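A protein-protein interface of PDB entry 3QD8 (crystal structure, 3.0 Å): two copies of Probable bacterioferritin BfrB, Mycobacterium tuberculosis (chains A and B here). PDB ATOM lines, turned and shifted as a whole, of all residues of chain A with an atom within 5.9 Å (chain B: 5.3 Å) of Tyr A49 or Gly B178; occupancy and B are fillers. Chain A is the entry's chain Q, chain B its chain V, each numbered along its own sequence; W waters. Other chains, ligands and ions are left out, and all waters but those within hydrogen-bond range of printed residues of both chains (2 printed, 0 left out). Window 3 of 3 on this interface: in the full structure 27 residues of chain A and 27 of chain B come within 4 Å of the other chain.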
ATOM      1  N   TYR A  29     -11.737   3.474  -6.874  1.00  0.00           N
ATOM      2  CA  TYR A  29     -11.011   2.510  -7.679  1.00  0.00           C
ATOM      3  C   TYR A  29     -11.792   2.144  -8.932  1.00  0.00           C
ATOM      4  O   TYR A  29     -11.222   2.109 -10.016  1.00  0.00           O
ATOM      5  CB  TYR A  29     -10.689   1.260  -6.868  1.00  0.00           C
ATOM      6  CG  TYR A  29      -9.440   1.375  -6.023  1.00  0.00           C
ATOM      7  CD1 TYR A  29      -8.395   2.196  -6.408  1.00  0.00           C
ATOM      8  CD2 TYR A  29      -9.295   0.641  -4.856  1.00  0.00           C
ATOM      9  CE1 TYR A  29      -7.250   2.298  -5.646  1.00  0.00           C
ATOM     10  CE2 TYR A  29      -8.155   0.736  -4.089  1.00  0.00           C
ATOM     11  CZ  TYR A  29      -7.137   1.567  -4.486  1.00  0.00           C
ATOM     12  OH  TYR A  29      -5.995   1.663  -3.726  1.00  0.00           O
ATOM     13  N   VAL A  30     -13.084   1.868  -8.786  1.00  0.00           N
ATOM     14  CA  VAL A  30     -13.922   1.597  -9.945  1.00  0.00           C
ATOM     15  C   VAL A  30     -13.788   2.750 -10.944  1.00  0.00           C
ATOM     16  O   VAL A  30     -13.627   2.552 -12.151  1.00  0.00           O
ATOM     17  CB  VAL A  30     -15.408   1.424  -9.556  1.00  0.00           C
ATOM     18  CG1 VAL A  30     -16.207   0.921 -10.740  1.00  0.00           C
ATOM     19  CG2 VAL A  30     -15.546   0.461  -8.415  1.00  0.00           C
ATOM     20  N   ALA A  33     -10.543   2.440 -12.550  1.00  0.00           N
ATOM     21  CA  ALA A  33     -10.578   1.293 -13.451  1.00  0.00           C
ATOM     22  C   ALA A  33     -11.286   1.656 -14.747  1.00  0.00           C
ATOM     23  O   ALA A  33     -10.757   1.445 -15.844  1.00  0.00           O
ATOM     24  CB  ALA A  33     -11.263   0.121 -12.791  1.00  0.00           C
ATOM     25  N   VAL A  34     -12.480   2.217 -14.614  1.00  0.00           N
ATOM     26  CA  VAL A  34     -13.261   2.628 -15.774  1.00  0.00           C
ATOM     27  C   VAL A  34     -12.510   3.658 -16.635  1.00  0.00           C
ATOM     28  O   VAL A  34     -12.609   3.641 -17.860  1.00  0.00           O
ATOM     29  CB  VAL A  34     -14.659   3.172 -15.364  1.00  0.00           C
ATOM     30  CG1 VAL A  34     -15.319   3.862 -16.525  1.00  0.00           C
ATOM     31  CG2 VAL A  34     -15.548   2.050 -14.871  1.00  0.00           C
ATOM     32  N   ASP A  37     -10.040   1.782 -18.611  1.00  0.00           N
ATOM     33  CA  ASP A  37     -10.764   0.958 -19.567  1.00  0.00           C
ATOM     34  C   ASP A  37     -11.053   1.797 -20.810  1.00  0.00           C
ATOM     35  O   ASP A  37     -10.859   1.350 -21.946  1.00  0.00           O
ATOM     36  CB  ASP A  37     -12.043   0.430 -18.920  1.00  0.00           C
ATOM     37  CG  ASP A  37     -12.662  -0.714 -19.679  1.00  0.00           C
ATOM     38  OD1 ASP A  37     -12.598  -0.729 -20.933  1.00  0.00           O
ATOM     39  OD2 ASP A  37     -13.235  -1.596 -19.008  1.00  0.00           O
ATOM     40  N   LEU A  44      -4.072  -2.352 -16.962  1.00  0.00           N
ATOM     41  CA  LEU A  44      -4.283  -1.460 -15.848  1.00  0.00           C
ATOM     42  C   LEU A  44      -5.732  -1.562 -15.345  1.00  0.00           C
ATOM     43  O   LEU A  44      -5.992  -1.691 -14.133  1.00  0.00           O
ATOM     44  CB  LEU A  44      -3.950  -0.029 -16.269  1.00  0.00           C
ATOM     45  CG  LEU A  44      -2.457   0.303 -16.160  1.00  0.00           C
ATOM     46  CD1 LEU A  44      -2.083   1.596 -16.866  1.00  0.00           C
ATOM     47  CD2 LEU A  44      -2.030   0.350 -14.688  1.00  0.00           C
ATOM     48  N   ALA A  45      -6.670  -1.509 -16.283  1.00  0.00           N
ATOM     49  CA  ALA A  45      -8.073  -1.517 -15.919  1.00  0.00           C
ATOM     50  C   ALA A  45      -8.425  -2.802 -15.163  1.00  0.00           C
ATOM     51  O   ALA A  45      -9.045  -2.754 -14.085  1.00  0.00           O
ATOM     52  CB  ALA A  45      -8.957  -1.332 -17.165  1.00  0.00           C
ATOM     53  N   LYS A  46      -8.019  -3.941 -15.730  1.00  0.00           N
ATOM     54  CA  LYS A  46      -8.355  -5.243 -15.149  1.00  0.00           C
ATOM     55  C   LYS A  46      -7.899  -5.291 -13.699  1.00  0.00           C
ATOM     56  O   LYS A  46      -8.590  -5.806 -12.805  1.00  0.00           O
ATOM     57  CB  LYS A  46      -7.724  -6.399 -15.941  1.00  0.00           C
ATOM     58  CG  LYS A  46      -7.959  -7.767 -15.286  1.00  0.00           C
ATOM     59  CD  LYS A  46      -7.450  -8.922 -16.133  1.00  0.00           C
ATOM     60  CE  LYS A  46      -6.096  -9.442 -15.657  1.00  0.00           C
ATOM     61  NZ  LYS A  46      -5.473 -10.352 -16.674  1.00  0.00           N
ATOM     62  N   HIS A  47      -6.720  -4.729 -13.476  1.00  0.00           N
ATOM     63  CA  HIS A  47      -6.149  -4.733 -12.150  1.00  0.00           C
ATOM     64  C   HIS A  47      -6.954  -3.876 -11.184  1.00  0.00           C
ATOM     65  O   HIS A  47      -7.254  -4.315 -10.080  1.00  0.00           O
ATOM     66  CB  HIS A  47      -4.707  -4.271 -12.180  1.00  0.00           C
ATOM     67  CG  HIS A  47      -4.102  -4.178 -10.822  1.00  0.00           C
ATOM     68  ND1 HIS A  47      -3.541  -5.267 -10.188  1.00  0.00           N
ATOM     69  CD2 HIS A  47      -4.004  -3.137  -9.956  1.00  0.00           C
ATOM     70  CE1 HIS A  47      -3.103  -4.893  -8.996  1.00  0.00           C
ATOM     71  NE2 HIS A  47      -3.377  -3.609  -8.828  1.00  0.00           N
ATOM     72  N   PHE A  48      -7.312  -2.662 -11.591  1.00  0.00           N
ATOM     73  CA  PHE A  48      -8.028  -1.778 -10.676  1.00  0.00           C
ATOM     74  C   PHE A  48      -9.503  -2.174 -10.474  1.00  0.00           C
ATOM     75  O   PHE A  48     -10.129  -1.831  -9.456  1.00  0.00           O
ATOM     76  CB  PHE A  48      -7.856  -0.305 -11.073  1.00  0.00           C
ATOM     77  CG  PHE A  48      -6.554   0.290 -10.613  1.00  0.00           C
ATOM     78  CD1 PHE A  48      -6.474   0.970  -9.408  1.00  0.00           C
ATOM     79  CD2 PHE A  48      -5.394   0.149 -11.381  1.00  0.00           C
ATOM     80  CE1 PHE A  48      -5.266   1.510  -8.975  1.00  0.00           C
ATOM     81  CE2 PHE A  48      -4.173   0.693 -10.958  1.00  0.00           C
ATOM     82  CZ  PHE A  48      -4.111   1.369  -9.756  1.00  0.00           C
ATOM     83  N   TYR A  49     -10.056  -2.903 -11.433  1.00  0.00           N
ATOM     84  CA  TYR A  49     -11.374  -3.485 -11.228  1.00  0.00           C
ATOM     85  C   TYR A  49     -11.254  -4.448 -10.057  1.00  0.00           C
ATOM     86  O   TYR A  49     -12.100  -4.478  -9.141  1.00  0.00           O
ATOM     87  CB  TYR A  49     -11.844  -4.233 -12.474  1.00  0.00           C
ATOM     88  CG  TYR A  49     -12.412  -3.347 -13.547  1.00  0.00           C
ATOM     89  CD1 TYR A  49     -13.490  -2.518 -13.289  1.00  0.00           C
ATOM     90  CD2 TYR A  49     -11.881  -3.352 -14.819  1.00  0.00           C
ATOM     91  CE1 TYR A  49     -14.017  -1.716 -14.266  1.00  0.00           C
ATOM     92  CE2 TYR A  49     -12.404  -2.553 -15.808  1.00  0.00           C
ATOM     93  CZ  TYR A  49     -13.473  -1.740 -15.527  1.00  0.00           C
ATOM     94  OH  TYR A  49     -13.988  -0.945 -16.525  1.00  0.00           O
ATOM     95  N   SER A  50     -10.171  -5.221 -10.101  1.00  0.00           N
ATOM     96  CA  SER A  50      -9.864  -6.188  -9.069  1.00  0.00           C
ATOM     97  C   SER A  50      -9.591  -5.485  -7.754  1.00  0.00           C
ATOM     98  O   SER A  50     -10.108  -5.869  -6.701  1.00  0.00           O
ATOM     99  CB  SER A  50      -8.646  -7.013  -9.474  1.00  0.00           C
ATOM    100  OG  SER A  50      -8.267  -7.873  -8.415  1.00  0.00           O
ATOM    101  N   GLN A  51      -8.769  -4.449  -7.838  1.00  0.00           N
ATOM    102  CA  GLN A  51      -8.410  -3.648  -6.692  1.00  0.00           C
ATOM    103  C   GLN A  51      -9.645  -3.097  -5.973  1.00  0.00           C
ATOM    104  O   GLN A  51      -9.689  -3.053  -4.732  1.00  0.00           O
ATOM    105  CB  GLN A  51      -7.511  -2.501  -7.134  1.00  0.00           C
ATOM    106  CG  GLN A  51      -6.789  -1.802  -5.978  1.00  0.00           C
ATOM    107  CD  GLN A  51      -5.683  -2.663  -5.380  1.00  0.00           C
ATOM    108  OE1 GLN A  51      -4.642  -2.908  -6.015  1.00  0.00           O
ATOM    109  NE2 GLN A  51      -5.902  -3.129  -4.151  1.00  0.00           N
ATOM    110  N   ALA A  52     -10.641  -2.677  -6.751  1.00  0.00           N
ATOM    111  CA  ALA A  52     -11.848  -2.108  -6.184  1.00  0.00           C
ATOM    112  C   ALA A  52     -12.609  -3.163  -5.413  1.00  0.00           C
ATOM    113  O   ALA A  52     -13.150  -2.899  -4.342  1.00  0.00           O
ATOM    114  CB  ALA A  52     -12.709  -1.509  -7.266  1.00  0.00           C
ATOM    115  N   VAL A  53     -12.639  -4.370  -5.951  1.00  0.00           N
ATOM    116  CA  VAL A  53     -13.321  -5.454  -5.268  1.00  0.00           C
ATOM    117  C   VAL A  53     -12.660  -5.793  -3.939  1.00  0.00           C
ATOM    118  O   VAL A  53     -13.344  -6.017  -2.939  1.00  0.00           O
ATOM    119  CB  VAL A  53     -13.409  -6.716  -6.128  1.00  0.00           C
ATOM    120  CG1 VAL A  53     -13.923  -7.859  -5.288  1.00  0.00           C
ATOM    121  CG2 VAL A  53     -14.329  -6.496  -7.311  1.00  0.00           C
ATOM    122  N   GLU A  54     -11.327  -5.830  -3.928  1.00  0.00           N
ATOM    123  CA  GLU A  54     -10.599  -6.110  -2.693  1.00  0.00           C
ATOM    124  C   GLU A  54     -10.847  -5.029  -1.644  1.00  0.00           C
ATOM    125  O   GLU A  54     -10.933  -5.324  -0.450  1.00  0.00           O
ATOM    126  CB  GLU A  54      -9.105  -6.320  -2.945  1.00  0.00           C
ATOM    127  CG  GLU A  54      -8.270  -6.591  -1.685  1.00  0.00           C
ATOM    128  CD  GLU A  54      -8.724  -7.819  -0.856  1.00  0.00           C
ATOM    129  OE1 GLU A  54      -9.546  -8.626  -1.336  1.00  0.00           O
ATOM    130  OE2 GLU A  54      -8.246  -7.981   0.292  1.00  0.00           O
ATOM    131  N   ARG B  56     -24.859  -4.693  -8.600  1.00  0.00           N
ATOM    132  CA  ARG B  56     -23.615  -4.059  -9.000  1.00  0.00           C
ATOM    133  C   ARG B  56     -23.288  -4.447 -10.438  1.00  0.00           C
ATOM    134  O   ARG B  56     -22.974  -3.588 -11.266  1.00  0.00           O
ATOM    135  CB  ARG B  56     -22.492  -4.467  -8.055  1.00  0.00           C
ATOM    136  CG  ARG B  56     -21.199  -3.686  -8.186  1.00  0.00           C
ATOM    137  CD  ARG B  56     -20.149  -4.285  -7.256  1.00  0.00           C
ATOM    138  NE  ARG B  56     -18.870  -3.590  -7.300  1.00  0.00           N
ATOM    139  CZ  ARG B  56     -17.862  -3.908  -8.111  1.00  0.00           C
ATOM    140  NH1 ARG B  56     -17.998  -4.918  -8.965  1.00  0.00           N
ATOM    141  NH2 ARG B  56     -16.725  -3.209  -8.062  1.00  0.00           N
ATOM    142  N   MET B  60     -22.420  -2.044 -13.741  1.00  0.00           N
ATOM    143  CA  MET B  60     -21.252  -2.193 -14.585  1.00  0.00           C
ATOM    144  C   MET B  60     -21.611  -2.548 -16.035  1.00  0.00           C
ATOM    145  O   MET B  60     -20.844  -2.275 -16.955  1.00  0.00           O
ATOM    146  CB  MET B  60     -20.321  -3.248 -13.981  1.00  0.00           C
ATOM    147  CG  MET B  60     -19.820  -2.860 -12.621  1.00  0.00           C
ATOM    148  SD  MET B  60     -19.180  -1.176 -12.716  1.00  0.00           S
ATOM    149  CE  MET B  60     -17.463  -1.488 -13.136  1.00  0.00           C
ATOM    150  N   GLN B  64     -20.435  -0.408 -19.161  1.00  0.00           N
ATOM    151  CA  GLN B  64     -19.859  -1.066 -20.323  1.00  0.00           C
ATOM    152  C   GLN B  64     -20.494  -0.598 -21.629  1.00  0.00           C
ATOM    153  O   GLN B  64     -19.803  -0.429 -22.648  1.00  0.00           O
ATOM    154  CB  GLN B  64     -19.998  -2.584 -20.191  1.00  0.00           C
ATOM    155  CG  GLN B  64     -19.275  -3.354 -21.272  1.00  0.00           C
ATOM    156  CD  GLN B  64     -17.784  -3.204 -21.191  1.00  0.00           C
ATOM    157  OE1 GLN B  64     -17.155  -3.683 -20.249  1.00  0.00           O
ATOM    158  NE2 GLN B  64     -17.207  -2.540 -22.174  1.00  0.00           N
ATOM    159  N   LEU B  67     -19.141   2.771 -22.488  1.00  0.00           N
ATOM    160  CA  LEU B  67     -17.774   2.485 -22.909  1.00  0.00           C
ATOM    161  C   LEU B  67     -17.736   2.012 -24.364  1.00  0.00           C
ATOM    162  O   LEU B  67     -16.988   2.578 -25.181  1.00  0.00           O
ATOM    163  CB  LEU B  67     -17.139   1.426 -22.015  1.00  0.00           C
ATOM    164  CG  LEU B  67     -16.581   1.880 -20.677  1.00  0.00           C
ATOM    165  CD1 LEU B  67     -15.955   0.699 -19.924  1.00  0.00           C
ATOM    166  CD2 LEU B  67     -15.581   2.997 -20.895  1.00  0.00           C
ATOM    167  N   HIS B 175     -22.290  -7.752 -21.471  1.00  0.00           N
ATOM    168  CA  HIS B 175     -21.048  -7.768 -20.722  1.00  0.00           C
ATOM    169  C   HIS B 175     -20.976  -6.670 -19.686  1.00  0.00           C
ATOM    170  O   HIS B 175     -21.502  -5.565 -19.869  1.00  0.00           O
ATOM    171  CB  HIS B 175     -19.827  -7.679 -21.615  1.00  0.00           C
ATOM    172  CG  HIS B 175     -18.545  -7.859 -20.863  1.00  0.00           C
ATOM    173  ND1 HIS B 175     -18.230  -9.034 -20.210  1.00  0.00           N
ATOM    174  CD2 HIS B 175     -17.515  -7.012 -20.634  1.00  0.00           C
ATOM    175  CE1 HIS B 175     -17.051  -8.908 -19.629  1.00  0.00           C
ATOM    176  NE2 HIS B 175     -16.594  -7.690 -19.871  1.00  0.00           N
ATOM    177  N   ALA B 176     -20.289  -6.984 -18.598  1.00  0.00           N
ATOM    178  CA  ALA B 176     -20.201  -6.080 -17.466  1.00  0.00           C
ATOM    179  C   ALA B 176     -18.772  -5.609 -17.260  1.00  0.00           C
ATOM    180  O   ALA B 176     -17.869  -6.432 -17.133  1.00  0.00           O
ATOM    181  CB  ALA B 176     -20.707  -6.774 -16.231  1.00  0.00           C
ATOM    182  N   ALA B 177     -18.564  -4.293 -17.253  1.00  0.00           N
ATOM    183  CA  ALA B 177     -17.233  -3.753 -17.029  1.00  0.00           C
ATOM    184  C   ALA B 177     -16.654  -4.468 -15.821  1.00  0.00           C
ATOM    185  O   ALA B 177     -17.320  -4.582 -14.778  1.00  0.00           O
ATOM    186  CB  ALA B 177     -17.291  -2.264 -16.787  1.00  0.00           C
ATOM    187  N   GLY B 178     -15.436  -4.980 -15.984  1.00  0.00           N
ATOM    188  CA  GLY B 178     -14.789  -5.759 -14.947  1.00  0.00           C
ATOM    189  C   GLY B 178     -15.072  -7.259 -14.933  1.00  0.00           C
ATOM    190  O   GLY B 178     -14.187  -8.041 -14.586  1.00  0.00           O
ATOM    191  N   GLY B 179     -16.297  -7.647 -15.304  1.00  0.00           N
ATOM    192  CA  GLY B 179     -16.768  -9.022 -15.268  1.00  0.00           C
ATOM    193  C   GLY B 179     -18.086  -9.166 -14.523  1.00  0.00           C
ATOM    194  O   GLY B 179     -18.774  -8.191 -14.279  1.00  0.00           O
ATOM    195  N   ARG B 180     -18.455 -10.388 -14.170  1.00  0.00           N
ATOM    196  CA  ARG B 180     -19.587 -10.602 -13.292  1.00  0.00           C
ATOM    197  C   ARG B 180     -19.000 -11.153 -12.006  1.00  0.00           C
ATOM    198  O   ARG B 180     -18.022 -11.896 -12.048  1.00  0.00           O
ATOM    199  CB  ARG B 180     -20.533 -11.646 -13.889  1.00  0.00           C
ATOM    200  CG  ARG B 180     -21.238 -11.232 -15.170  1.00  0.00           C
ATOM    201  CD  ARG B 180     -22.689 -10.796 -14.979  1.00  0.00           C
ATOM    202  NE  ARG B 180     -23.530 -11.837 -14.383  1.00  0.00           N
ATOM    203  CZ  ARG B 180     -24.851 -11.938 -14.549  1.00  0.00           C
ATOM    204  NH1 ARG B 180     -25.505 -11.083 -15.319  1.00  0.00           N
ATOM    205  NH2 ARG B 180     -25.524 -12.910 -13.952  1.00  0.00           N
HETATM  206  O   HOH W   1     -14.308  -4.420 -19.381  1.00  0.00           O
HETATM  207  O   HOH W   2     -11.116  -7.933 -13.524  1.00  0.00           O
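The side-chain carboxylate (OD2) of Asp A37 is in hydrogen-bond range of the side-chain hydroxyl (OH) of Tyr A49 (2.7 Å). O of Met B60 lies within hydrogen-bond range of N of Ala B177, at 3.1 Å. The side-chain amide oxygen (OE1) of Gln B64 lies close to the backbone NH (N) of Ala B177.
Among the printed residues, pairs that only touch across the chains: Tyr A49 with Ala B177, Asp A37 with Leu B67, Val A30 with Met B60, Tyr A49 with Met B60, Tyr A49 with Gly B178 and Val A30 with Arg B56.
Tyr A49 touches three residues of chain B. Of the printed residues of chain A, Arg B56 touches Val A30. Of the printed residues of chain A, Met B60 touches Val A30 (3.6 Å) and Tyr A49 (3.6 Å). Of the printed residues of chain A, Leu B67 touches Asp A37 (3.6 Å). Of the printed residues of chain A, Ala B177 touches Tyr A49 (3.6 Å). Lys A46 touches none of the printed residues of chain B. Gln B64 touches none of the printed residues of chain A.
Hydrophobic or aromatic side chains of chain A that line the printed part of chain B: Val A30 and Tyr A49. Hydrophobic or aromatic side chains of chain B within 4 Å of the printed part of chain A: Met B60, Leu B67 and Ala B177. Along chain B the printed residues that touch a printed residue of chain A span positions 56 to 178. Among the printed residues, no Asp or Glu carboxylate lies within 4 Å of a Lys or Arg side-chain nitrogen of the other chain.
No position is printed for both chains. Of the 6 pairs that touch across the chains among the printed residues, none has its exchanged pair printed and touching as well.
Water W1 lies within hydrogen-bond range of OD2 of Asp A37 and OE1 of Gln B64. Water W2 lies within hydrogen-bond range of the backbone carbonyl oxygen (O) of Gly B178 (3.3 Å) and the backbone carbonyl oxygen (O) of Lys A46 (3.4 Å).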
